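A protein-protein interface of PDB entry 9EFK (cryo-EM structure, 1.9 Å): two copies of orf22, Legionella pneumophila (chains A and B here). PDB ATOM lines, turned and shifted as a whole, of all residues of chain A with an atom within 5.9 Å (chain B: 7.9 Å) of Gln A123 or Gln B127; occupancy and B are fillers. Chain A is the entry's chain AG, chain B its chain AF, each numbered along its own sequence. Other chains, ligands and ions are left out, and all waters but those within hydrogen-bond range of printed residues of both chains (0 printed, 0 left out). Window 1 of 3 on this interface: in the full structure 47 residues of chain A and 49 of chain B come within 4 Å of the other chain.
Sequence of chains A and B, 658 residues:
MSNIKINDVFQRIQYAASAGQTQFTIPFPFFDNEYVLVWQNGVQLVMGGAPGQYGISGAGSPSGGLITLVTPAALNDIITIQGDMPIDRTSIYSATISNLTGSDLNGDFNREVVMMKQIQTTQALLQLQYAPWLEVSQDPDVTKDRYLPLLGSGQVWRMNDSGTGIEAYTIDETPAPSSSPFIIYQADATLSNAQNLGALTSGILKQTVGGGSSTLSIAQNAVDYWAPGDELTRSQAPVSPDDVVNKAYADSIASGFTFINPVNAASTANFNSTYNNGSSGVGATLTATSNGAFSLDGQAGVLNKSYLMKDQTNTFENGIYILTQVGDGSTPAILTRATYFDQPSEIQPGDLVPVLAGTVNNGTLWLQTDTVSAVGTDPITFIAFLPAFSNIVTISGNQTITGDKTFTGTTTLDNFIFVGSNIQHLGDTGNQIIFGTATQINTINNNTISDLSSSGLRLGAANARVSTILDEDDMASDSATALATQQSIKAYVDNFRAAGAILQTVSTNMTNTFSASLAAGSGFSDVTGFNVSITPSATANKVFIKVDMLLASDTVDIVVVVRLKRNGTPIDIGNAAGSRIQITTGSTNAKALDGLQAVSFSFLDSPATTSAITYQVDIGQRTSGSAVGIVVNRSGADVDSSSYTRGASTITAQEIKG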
ATOM      1  N   GLN A 118     -27.961  12.958  -5.177  1.00  0.00           N
ATOM      2  CA  GLN A 118     -28.241  12.941  -3.745  1.00  0.00           C
ATOM      3  C   GLN A 118     -27.144  13.644  -2.955  1.00  0.00           C
ATOM      4  O   GLN A 118     -27.429  14.344  -1.980  1.00  0.00           O
ATOM      5  CB  GLN A 118     -28.425  11.507  -3.260  1.00  0.00           C
ATOM      6  CG  GLN A 118     -29.675  10.854  -3.800  1.00  0.00           C
ATOM      7  CD  GLN A 118     -29.800   9.406  -3.404  1.00  0.00           C
ATOM      8  OE1 GLN A 118     -28.955   8.870  -2.695  1.00  0.00           O
ATOM      9  NE2 GLN A 118     -30.858   8.763  -3.865  1.00  0.00           N
ATOM     10  N   ILE A 119     -25.886  13.461  -3.355  1.00  0.00           N
ATOM     11  CA  ILE A 119     -24.787  14.180  -2.716  1.00  0.00           C
ATOM     12  C   ILE A 119     -24.926  15.676  -2.953  1.00  0.00           C
ATOM     13  O   ILE A 119     -24.791  16.487  -2.031  1.00  0.00           O
ATOM     14  CB  ILE A 119     -23.435  13.652  -3.225  1.00  0.00           C
ATOM     15  CG1 ILE A 119     -23.210  12.217  -2.755  1.00  0.00           C
ATOM     16  CG2 ILE A 119     -22.304  14.547  -2.766  1.00  0.00           C
ATOM     17  CD1 ILE A 119     -21.992  11.577  -3.351  1.00  0.00           C
ATOM     18  N   GLN A 120     -25.216  16.063  -4.193  1.00  0.00           N
ATOM     19  CA  GLN A 120     -25.307  17.480  -4.523  1.00  0.00           C
ATOM     20  C   GLN A 120     -26.568  18.117  -3.952  1.00  0.00           C
ATOM     21  O   GLN A 120     -26.591  19.327  -3.710  1.00  0.00           O
ATOM     22  CB  GLN A 120     -25.240  17.658  -6.037  1.00  0.00           C
ATOM     23  CG  GLN A 120     -25.037  19.086  -6.494  1.00  0.00           C
ATOM     24  CD  GLN A 120     -26.339  19.811  -6.716  1.00  0.00           C
ATOM     25  OE1 GLN A 120     -27.374  19.191  -6.934  1.00  0.00           O
ATOM     26  NE2 GLN A 120     -26.298  21.132  -6.660  1.00  0.00           N
ATOM     27  N   THR A 121     -27.620  17.330  -3.732  1.00  0.00           N
ATOM     28  CA  THR A 121     -28.820  17.860  -3.092  1.00  0.00           C
ATOM     29  C   THR A 121     -28.547  18.236  -1.642  1.00  0.00           C
ATOM     30  O   THR A 121     -29.007  19.281  -1.170  1.00  0.00           O
ATOM     31  CB  THR A 121     -29.957  16.844  -3.182  1.00  0.00           C
ATOM     32  OG1 THR A 121     -30.371  16.716  -4.545  1.00  0.00           O
ATOM     33  CG2 THR A 121     -31.138  17.283  -2.347  1.00  0.00           C
ATOM     34  N   THR A 122     -27.804  17.396  -0.922  1.00  0.00           N
ATOM     35  CA  THR A 122     -27.403  17.737   0.436  1.00  0.00           C
ATOM     36  C   THR A 122     -26.494  18.956   0.444  1.00  0.00           C
ATOM     37  O   THR A 122     -26.642  19.847   1.285  1.00  0.00           O
ATOM     38  CB  THR A 122     -26.713  16.538   1.090  1.00  0.00           C
ATOM     39  OG1 THR A 122     -27.670  15.496   1.303  1.00  0.00           O
ATOM     40  CG2 THR A 122     -26.093  16.921   2.415  1.00  0.00           C
ATOM     41  N   GLN A 123     -25.563  19.021  -0.505  1.00  0.00           N
ATOM     42  CA  GLN A 123     -24.639  20.145  -0.580  1.00  0.00           C
ATOM     43  C   GLN A 123     -25.372  21.455  -0.840  1.00  0.00           C
ATOM     44  O   GLN A 123     -25.073  22.476  -0.214  1.00  0.00           O
ATOM     45  CB  GLN A 123     -23.607  19.877  -1.672  1.00  0.00           C
ATOM     46  CG  GLN A 123     -22.490  20.884  -1.759  1.00  0.00           C
ATOM     47  CD  GLN A 123     -21.471  20.516  -2.813  1.00  0.00           C
ATOM     48  OE1 GLN A 123     -21.795  20.408  -3.988  1.00  0.00           O
ATOM     49  NE2 GLN A 123     -20.235  20.311  -2.392  1.00  0.00           N
ATOM     50  N   ALA A 124     -26.340  21.446  -1.756  1.00  0.00           N
ATOM     51  CA  ALA A 124     -27.011  22.676  -2.158  1.00  0.00           C
ATOM     52  C   ALA A 124     -28.039  23.144  -1.135  1.00  0.00           C
ATOM     53  O   ALA A 124     -28.171  24.348  -0.899  1.00  0.00           O
ATOM     54  CB  ALA A 124     -27.677  22.489  -3.518  1.00  0.00           C
ATOM     55  N   LEU A 125     -28.780  22.224  -0.524  1.00  0.00           N
ATOM     56  CA  LEU A 125     -29.901  22.597   0.326  1.00  0.00           C
ATOM     57  C   LEU A 125     -29.623  22.501   1.815  1.00  0.00           C
ATOM     58  O   LEU A 125     -30.245  23.229   2.586  1.00  0.00           O
ATOM     59  CB  LEU A 125     -31.125  21.734   0.002  1.00  0.00           C
ATOM     60  CG  LEU A 125     -31.724  21.903  -1.391  1.00  0.00           C
ATOM     61  CD1 LEU A 125     -32.914  20.987  -1.566  1.00  0.00           C
ATOM     62  CD2 LEU A 125     -32.128  23.341  -1.621  1.00  0.00           C
ATOM     63  N   LEU A 126     -28.716  21.635   2.249  1.00  0.00           N
ATOM     64  CA  LEU A 126     -28.556  21.369   3.668  1.00  0.00           C
ATOM     65  C   LEU A 126     -27.195  21.746   4.228  1.00  0.00           C
ATOM     66  O   LEU A 126     -26.955  21.514   5.414  1.00  0.00           O
ATOM     67  CB  LEU A 126     -28.823  19.886   3.962  1.00  0.00           C
ATOM     68  CG  LEU A 126     -30.217  19.365   3.623  1.00  0.00           C
ATOM     69  CD1 LEU A 126     -30.279  17.864   3.795  1.00  0.00           C
ATOM     70  CD2 LEU A 126     -31.260  20.041   4.483  1.00  0.00           C
ATOM     71  N   GLN A 127     -26.299  22.314   3.433  1.00  0.00           N
ATOM     72  CA  GLN A 127     -24.947  22.584   3.891  1.00  0.00           C
ATOM     73  C   GLN A 127     -24.593  24.054   3.723  1.00  0.00           C
ATOM     74  O   GLN A 127     -25.194  24.774   2.926  1.00  0.00           O
ATOM     75  CB  GLN A 127     -23.927  21.723   3.148  1.00  0.00           C
ATOM     76  CG  GLN A 127     -23.924  20.274   3.566  1.00  0.00           C
ATOM     77  CD  GLN A 127     -22.738  19.524   3.021  1.00  0.00           C
ATOM     78  OE1 GLN A 127     -22.389  19.660   1.856  1.00  0.00           O
ATOM     79  NE2 GLN A 127     -22.105  18.733   3.869  1.00  0.00           N
ATOM     80  N   LEU A 128     -23.599  24.485   4.487  1.00  0.00           N
ATOM     81  CA  LEU A 128     -23.096  25.848   4.430  1.00  0.00           C
ATOM     82  C   LEU A 128     -21.946  25.954   3.442  1.00  0.00           C
ATOM     83  O   LEU A 128     -21.161  25.020   3.272  1.00  0.00           O
ATOM     84  CB  LEU A 128     -22.612  26.305   5.801  1.00  0.00           C
ATOM     85  CG  LEU A 128     -23.497  26.029   7.005  1.00  0.00           C
ATOM     86  CD1 LEU A 128     -22.709  26.324   8.256  1.00  0.00           C
ATOM     87  CD2 LEU A 128     -24.738  26.878   6.940  1.00  0.00           C
ATOM     88  N   GLN A 129     -21.842  27.113   2.803  1.00  0.00           N
ATOM     89  CA  GLN A 129     -20.716  27.397   1.929  1.00  0.00           C
ATOM     90  C   GLN A 129     -20.520  28.900   1.836  1.00  0.00           C
ATOM     91  O   GLN A 129     -21.449  29.682   2.034  1.00  0.00           O
ATOM     92  CB  GLN A 129     -20.918  26.810   0.530  1.00  0.00           C
ATOM     93  CG  GLN A 129     -21.940  27.552  -0.301  1.00  0.00           C
ATOM     94  CD  GLN A 129     -21.959  27.098  -1.740  1.00  0.00           C
ATOM     95  OE1 GLN A 129     -21.353  27.723  -2.606  1.00  0.00           O
ATOM     96  NE2 GLN A 129     -22.656  26.003  -2.006  1.00  0.00           N
ATOM     97  N   TYR A 130     -19.291  29.298   1.531  1.00  0.00           N
ATOM     98  CA  TYR A 130     -19.035  30.677   1.156  1.00  0.00           C
ATOM     99  C   TYR A 130     -19.670  30.970  -0.194  1.00  0.00           C
ATOM    100  O   TYR A 130     -19.835  30.083  -1.030  1.00  0.00           O
ATOM    101  CB  TYR A 130     -17.536  30.953   1.089  1.00  0.00           C
ATOM    102  CG  TYR A 130     -16.831  30.823   2.411  1.00  0.00           C
ATOM    103  CD1 TYR A 130     -17.090  31.709   3.439  1.00  0.00           C
ATOM    104  CD2 TYR A 130     -15.902  29.822   2.631  1.00  0.00           C
ATOM    105  CE1 TYR A 130     -16.452  31.600   4.644  1.00  0.00           C
ATOM    106  CE2 TYR A 130     -15.257  29.707   3.836  1.00  0.00           C
ATOM    107  CZ  TYR A 130     -15.540  30.600   4.840  1.00  0.00           C
ATOM    108  OH  TYR A 130     -14.908  30.504   6.048  1.00  0.00           O
ATOM    109  N   ASP A 145      -9.548  29.500   6.322  1.00  0.00           N
ATOM    110  CA  ASP A 145     -10.976  29.770   6.312  1.00  0.00           C
ATOM    111  C   ASP A 145     -11.837  28.517   6.323  1.00  0.00           C
ATOM    112  O   ASP A 145     -13.053  28.628   6.483  1.00  0.00           O
ATOM    113  CB  ASP A 145     -11.344  30.608   5.087  1.00  0.00           C
ATOM    114  CG  ASP A 145     -10.899  32.046   5.210  1.00  0.00           C
ATOM    115  OD1 ASP A 145     -11.135  32.654   6.273  1.00  0.00           O
ATOM    116  OD2 ASP A 145     -10.310  32.567   4.244  1.00  0.00           O
ATOM    117  N   ARG A 146     -11.251  27.332   6.179  1.00  0.00           N
ATOM    118  CA  ARG A 146     -12.044  26.149   5.894  1.00  0.00           C
ATOM    119  C   ARG A 146     -11.935  25.029   6.917  1.00  0.00           C
ATOM    120  O   ARG A 146     -12.841  24.195   6.973  1.00  0.00           O
ATOM    121  CB  ARG A 146     -11.686  25.600   4.506  1.00  0.00           C
ATOM    122  CG  ARG A 146     -12.077  26.541   3.379  1.00  0.00           C
ATOM    123  CD  ARG A 146     -11.678  26.003   2.023  1.00  0.00           C
ATOM    124  NE  ARG A 146     -10.260  26.186   1.744  1.00  0.00           N
ATOM    125  CZ  ARG A 146      -9.777  27.047   0.862  1.00  0.00           C
ATOM    126  NH1 ARG A 146     -10.573  27.820   0.147  1.00  0.00           N
ATOM    127  NH2 ARG A 146      -8.464  27.125   0.682  1.00  0.00           N
ATOM    128  N   ILE B  87     -26.939  17.920 -13.014  1.00  0.00           N
ATOM    129  CA  ILE B  87     -26.699  16.503 -12.756  1.00  0.00           C
ATOM    130  C   ILE B  87     -27.959  15.764 -13.186  1.00  0.00           C
ATOM    131  O   ILE B  87     -28.917  15.627 -12.428  1.00  0.00           O
ATOM    132  CB  ILE B  87     -26.345  16.241 -11.296  1.00  0.00           C
ATOM    133  CG1 ILE B  87     -25.071  16.991 -10.918  1.00  0.00           C
ATOM    134  CG2 ILE B  87     -26.170  14.755 -11.048  1.00  0.00           C
ATOM    135  CD1 ILE B  87     -24.621  16.737  -9.513  1.00  0.00           C
ATOM    136  N   MET B 115     -19.091  16.221 -13.316  1.00  0.00           N
ATOM    137  CA  MET B 115     -20.073  16.456 -12.262  1.00  0.00           C
ATOM    138  C   MET B 115     -19.447  16.285 -10.886  1.00  0.00           C
ATOM    139  O   MET B 115     -19.628  17.125 -10.000  1.00  0.00           O
ATOM    140  CB  MET B 115     -21.258  15.504 -12.418  1.00  0.00           C
ATOM    141  CG  MET B 115     -22.134  15.740 -13.624  1.00  0.00           C
ATOM    142  SD  MET B 115     -23.312  14.389 -13.817  1.00  0.00           S
ATOM    143  CE  MET B 115     -24.208  14.910 -15.267  1.00  0.00           C
ATOM    144  N   MET B 116     -18.700  15.198 -10.691  1.00  0.00           N
ATOM    145  CA  MET B 116     -18.066  14.961  -9.399  1.00  0.00           C
ATOM    146  C   MET B 116     -17.010  16.012  -9.103  1.00  0.00           C
ATOM    147  O   MET B 116     -16.828  16.410  -7.949  1.00  0.00           O
ATOM    148  CB  MET B 116     -17.456  13.561  -9.359  1.00  0.00           C
ATOM    149  CG  MET B 116     -18.463  12.464  -9.082  1.00  0.00           C
ATOM    150  SD  MET B 116     -17.733  10.831  -8.886  1.00  0.00           S
ATOM    151  CE  MET B 116     -17.091  10.542 -10.525  1.00  0.00           C
ATOM    152  N   GLN B 118     -17.091  19.142 -10.018  1.00  0.00           N
ATOM    153  CA  GLN B 118     -17.783  20.348  -9.574  1.00  0.00           C
ATOM    154  C   GLN B 118     -18.213  20.239  -8.118  1.00  0.00           C
ATOM    155  O   GLN B 118     -18.097  21.207  -7.361  1.00  0.00           O
ATOM    156  CB  GLN B 118     -18.985  20.626 -10.471  1.00  0.00           C
ATOM    157  CG  GLN B 118     -18.608  21.135 -11.842  1.00  0.00           C
ATOM    158  CD  GLN B 118     -19.797  21.294 -12.755  1.00  0.00           C
ATOM    159  OE1 GLN B 118     -20.934  21.060 -12.360  1.00  0.00           O
ATOM    160  NE2 GLN B 118     -19.539  21.681 -13.992  1.00  0.00           N
ATOM    161  N   ILE B 119     -18.712  19.073  -7.707  1.00  0.00           N
ATOM    162  CA  ILE B 119     -19.085  18.872  -6.309  1.00  0.00           C
ATOM    163  C   ILE B 119     -17.858  18.966  -5.414  1.00  0.00           C
ATOM    164  O   ILE B 119     -17.878  19.613  -4.364  1.00  0.00           O
ATOM    165  CB  ILE B 119     -19.801  17.524  -6.128  1.00  0.00           C
ATOM    166  CG1 ILE B 119     -21.127  17.511  -6.881  1.00  0.00           C
ATOM    167  CG2 ILE B 119     -20.028  17.235  -4.656  1.00  0.00           C
ATOM    168  CD1 ILE B 119     -21.825  16.183  -6.834  1.00  0.00           C
ATOM    169  N   GLN B 120     -16.770  18.317  -5.821  1.00  0.00           N
ATOM    170  CA  GLN B 120     -15.566  18.313  -5.003  1.00  0.00           C
ATOM    171  C   GLN B 120     -14.899  19.683  -4.968  1.00  0.00           C
ATOM    172  O   GLN B 120     -14.302  20.049  -3.954  1.00  0.00           O
ATOM    173  CB  GLN B 120     -14.600  17.250  -5.516  1.00  0.00           C
ATOM    174  CG  GLN B 120     -13.473  16.912  -4.566  1.00  0.00           C
ATOM    175  CD  GLN B 120     -12.246  17.756  -4.801  1.00  0.00           C
ATOM    176  OE1 GLN B 120     -12.059  18.305  -5.882  1.00  0.00           O
ATOM    177  NE2 GLN B 120     -11.400  17.865  -3.790  1.00  0.00           N
ATOM    178  N   THR B 121     -14.981  20.449  -6.056  1.00  0.00           N
ATOM    179  CA  THR B 121     -14.422  21.795  -6.050  1.00  0.00           C
ATOM    180  C   THR B 121     -15.134  22.675  -5.035  1.00  0.00           C
ATOM    181  O   THR B 121     -14.494  23.446  -4.314  1.00  0.00           O
ATOM    182  CB  THR B 121     -14.507  22.414  -7.445  1.00  0.00           C
ATOM    183  OG1 THR B 121     -13.682  21.673  -8.348  1.00  0.00           O
ATOM    184  CG2 THR B 121     -14.033  23.851  -7.418  1.00  0.00           C
ATOM    185  N   THR B 122     -16.459  22.565  -4.958  1.00  0.00           N
ATOM    186  CA  THR B 122     -17.208  23.314  -3.959  1.00  0.00           C
ATOM    187  C   THR B 122     -16.803  22.909  -2.548  1.00  0.00           C
ATOM    188  O   THR B 122     -16.558  23.764  -1.694  1.00  0.00           O
ATOM    189  CB  THR B 122     -18.707  23.109  -4.166  1.00  0.00           C
ATOM    190  OG1 THR B 122     -19.121  23.778  -5.361  1.00  0.00           O
ATOM    191  CG2 THR B 122     -19.492  23.657  -2.990  1.00  0.00           C
ATOM    192  N   GLN B 123     -16.706  21.608  -2.283  1.00  0.00           N
ATOM    193  CA  GLN B 123     -16.407  21.184  -0.923  1.00  0.00           C
ATOM    194  C   GLN B 123     -14.943  21.374  -0.553  1.00  0.00           C
ATOM    195  O   GLN B 123     -14.630  21.462   0.637  1.00  0.00           O
ATOM    196  CB  GLN B 123     -16.830  19.730  -0.707  1.00  0.00           C
ATOM    197  CG  GLN B 123     -15.903  18.690  -1.258  1.00  0.00           C
ATOM    198  CD  GLN B 123     -16.307  17.283  -0.843  1.00  0.00           C
ATOM    199  OE1 GLN B 123     -17.390  17.070  -0.306  1.00  0.00           O
ATOM    200  NE2 GLN B 123     -15.431  16.320  -1.089  1.00  0.00           N
ATOM    201  N   ALA B 124     -14.047  21.470  -1.529  1.00  0.00           N
ATOM    202  CA  ALA B 124     -12.642  21.703  -1.228  1.00  0.00           C
ATOM    203  C   ALA B 124     -12.303  23.177  -1.064  1.00  0.00           C
ATOM    204  O   ALA B 124     -11.415  23.510  -0.274  1.00  0.00           O
ATOM    205  CB  ALA B 124     -11.756  21.106  -2.322  1.00  0.00           C
ATOM    206  N   LEU B 125     -12.985  24.070  -1.781  1.00  0.00           N
ATOM    207  CA  LEU B 125     -12.634  25.481  -1.781  1.00  0.00           C
ATOM    208  C   LEU B 125     -13.658  26.384  -1.114  1.00  0.00           C
ATOM    209  O   LEU B 125     -13.291  27.472  -0.667  1.00  0.00           O
ATOM    210  CB  LEU B 125     -12.422  25.977  -3.218  1.00  0.00           C
ATOM    211  CG  LEU B 125     -11.280  25.362  -4.017  1.00  0.00           C
ATOM    212  CD1 LEU B 125     -11.279  25.911  -5.426  1.00  0.00           C
ATOM    213  CD2 LEU B 125      -9.951  25.621  -3.338  1.00  0.00           C
ATOM    214  N   LEU B 126     -14.917  25.975  -1.028  1.00  0.00           N
ATOM    215  CA  LEU B 126     -15.969  26.864  -0.568  1.00  0.00           C
ATOM    216  C   LEU B 126     -16.710  26.371   0.664  1.00  0.00           C
ATOM    217  O   LEU B 126     -17.635  27.050   1.112  1.00  0.00           O
ATOM    218  CB  LEU B 126     -16.983  27.111  -1.690  1.00  0.00           C
ATOM    219  CG  LEU B 126     -16.464  27.763  -2.969  1.00  0.00           C
ATOM    220  CD1 LEU B 126     -17.547  27.780  -4.022  1.00  0.00           C
ATOM    221  CD2 LEU B 126     -15.974  29.166  -2.690  1.00  0.00           C
ATOM    222  N   GLN B 127     -16.342  25.229   1.231  1.00  0.00           N
ATOM    223  CA  GLN B 127     -17.082  24.676   2.355  1.00  0.00           C
ATOM    224  C   GLN B 127     -16.170  24.461   3.552  1.00  0.00           C
ATOM    225  O   GLN B 127     -14.945  24.439   3.436  1.00  0.00           O
ATOM    226  CB  GLN B 127     -17.764  23.359   1.982  1.00  0.00           C
ATOM    227  CG  GLN B 127     -18.900  23.528   1.004  1.00  0.00           C
ATOM    228  CD  GLN B 127     -19.776  22.304   0.915  1.00  0.00           C
ATOM    229  OE1 GLN B 127     -19.436  21.336   0.250  1.00  0.00           O
ATOM    230  NE2 GLN B 127     -20.914  22.343   1.588  1.00  0.00           N
ATOM    231  N   LEU B 128     -16.797  24.322   4.714  1.00  0.00           N
ATOM    232  CA  LEU B 128     -16.098  24.058   5.959  1.00  0.00           C
ATOM    233  C   LEU B 128     -16.043  22.562   6.227  1.00  0.00           C
ATOM    234  O   LEU B 128     -16.916  21.802   5.804  1.00  0.00           O
ATOM    235  CB  LEU B 128     -16.792  24.750   7.129  1.00  0.00           C
ATOM    236  CG  LEU B 128     -17.164  26.220   6.989  1.00  0.00           C
ATOM    237  CD1 LEU B 128     -18.009  26.634   8.166  1.00  0.00           C
ATOM    238  CD2 LEU B 128     -15.921  27.064   6.902  1.00  0.00           C
ATOM    239  N   GLN B 129     -15.007  22.147   6.946  1.00  0.00           N
ATOM    240  CA  GLN B 129     -14.891  20.760   7.363  1.00  0.00           C
ATOM    241  C   GLN B 129     -13.923  20.676   8.528  1.00  0.00           C
ATOM    242  O   GLN B 129     -13.060  21.537   8.698  1.00  0.00           O
ATOM    243  CB  GLN B 129     -14.414  19.862   6.219  1.00  0.00           C
ATOM    244  CG  GLN B 129     -12.963  20.051   5.855  1.00  0.00           C
ATOM    245  CD  GLN B 129     -12.423  18.907   5.035  1.00  0.00           C
ATOM    246  OE1 GLN B 129     -11.588  18.136   5.500  1.00  0.00           O
ATOM    247  NE2 GLN B 129     -12.895  18.791   3.806  1.00  0.00           N
ATOM    248  N   TYR B 130     -14.082  19.632   9.331  1.00  0.00           N
ATOM    249  CA  TYR B 130     -13.084  19.323  10.337  1.00  0.00           C
ATOM    250  C   TYR B 130     -11.817  18.819   9.663  1.00  0.00           C
ATOM    251  O   TYR B 130     -11.856  18.264   8.564  1.00  0.00           O
ATOM    252  CB  TYR B 130     -13.615  18.277  11.311  1.00  0.00           C
ATOM    253  CG  TYR B 130     -14.774  18.755  12.144  1.00  0.00           C
ATOM    254  CD1 TYR B 130     -14.586  19.689  13.148  1.00  0.00           C
ATOM    255  CD2 TYR B 130     -16.054  18.276  11.930  1.00  0.00           C
ATOM    256  CE1 TYR B 130     -15.634  20.129  13.909  1.00  0.00           C
ATOM    257  CE2 TYR B 130     -17.108  18.709  12.691  1.00  0.00           C
ATOM    258  CZ  TYR B 130     -16.892  19.635  13.679  1.00  0.00           C
ATOM    259  OH  TYR B 130     -17.935  20.078  14.444  1.00  0.00           O
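The side-chain hydroxyl (OH) of Tyr A130 is in hydrogen-bond range of the backbone carbonyl oxygen (O) of Asp A145. OG1 of Thr B122 sits at hydrogen-bond distance from O of Gln B118, 3.4 Å away. The backbone carbonyl oxygen of Thr A122 lies within hydrogen-bond range of the backbone NH of Gln A127 (3.3 Å). The backbone NH (N) of Gln B127 sits at hydrogen-bond distance from the backbone carbonyl oxygen (O) of Thr B122 (3.3 Å).
Thr A121 touches none of the printed residues of chain B. Of chain B, only Ile B119 (3.2 Å), Thr B122 (3.5 Å), Gln B123 (3.8 Å) and Gln B127 (2.9 Å) come within 4 Å of Gln A123. No residue of chain B comes within 4 Å of Ala A124. Leu A126 touches none of the printed residues of chain B. Printed residues of chain B within 4 Å of Asp A145: Leu B128. Of the printed residues of chain A, Ile B119 touches Ile A119, Gln A120 and Gln A123. Of the printed residues of chain A, Leu B125 touches Arg A146 (2.9 Å). The nearest residue of chain B that does not touch Gln A123 is Gln B118 (5.1 Å). The nearest residue of chain A that does not touch Gln B127 is Tyr A130 (4.8 Å). The nearest printed residue of chain A that does not touch Gln B123 is Arg A146 (5.6 Å).
Hydrophobic or aromatic side chains of chain A that line the printed part of chain B: Ile A119 and Tyr A130. Among the printed residues, 19 pairs touch across the chains. Among the printed residues, no Asp or Glu carboxylate lies within 4 Å of a Lys or Arg side-chain nitrogen of the other chain.
OE1 of Gln B127 lies within hydrogen-bond range of NE2 of Gln A123 (2.9 Å). O of Leu B126 sits at hydrogen-bond distance from N of Tyr A130 (2.8 Å). The side-chain amide oxygen (OE1) of Gln A127 is in hydrogen-bond range of the side-chain amide nitrogen (NE2) of Gln B127 (3.1 Å). The backbone carbonyl oxygen of Leu B125 is in hydrogen-bond range of the guanidinium group of Arg A146 (2.9 Å). The backbone carbonyl oxygen (O) of Arg A146 lies within hydrogen-bond range of the backbone NH (N) of Gln B129, at 3.0 Å. O of Leu A128 lies within hydrogen-bond range of NE2 of Gln B127 (3.2 Å). O of Ile B119 sits at hydrogen-bond distance from NE2 of Gln A123 (3.2 Å).
Ile B119 touches its own counterpart, Ile A119. Gln A123 touches Thr B122, but with the chains exchanged Thr A122 does not touch Gln B123 (9.1 Å). Gln A129 touches Gln B127, but with the chains exchanged Gln A127 does not touch Gln B129 (8.1 Å). Tyr A130 touches Leu B128, but with the chains exchanged Leu A128 does not touch Tyr B130 (10.0 Å). Positions printed for both chains: 118, 119, 120, 121, 122, 123, 124, 125, 126, 127, 128, 129 and 130. Of the 19 pairs that touch across the chains among the printed residues, 3 have their exchanged pair printed and touching as well.
CG2 of Ile B119 touches CG2 of Ile A119, at 3.997 Å. Gln A120 touches Ile B87 (CB to CD1, 3.6 Å). CB of Gln A120 touches CD1 of Ile B119, at 3.8 Å. CG2 of Thr B122 touches NE2 of Gln A123, 3.5 Å away. Gln B123 touches Gln A123. Gln A129 touches Leu B126. Leu B128 touches Tyr A130 (CD2 to OH, 3.7 Å). O of Asp A145 touches CD2 of Leu B128 (3.3 Å). CD of Arg A146 touches O of Ala B124, 3.4 Å away. Arg A146 touches Leu B128.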
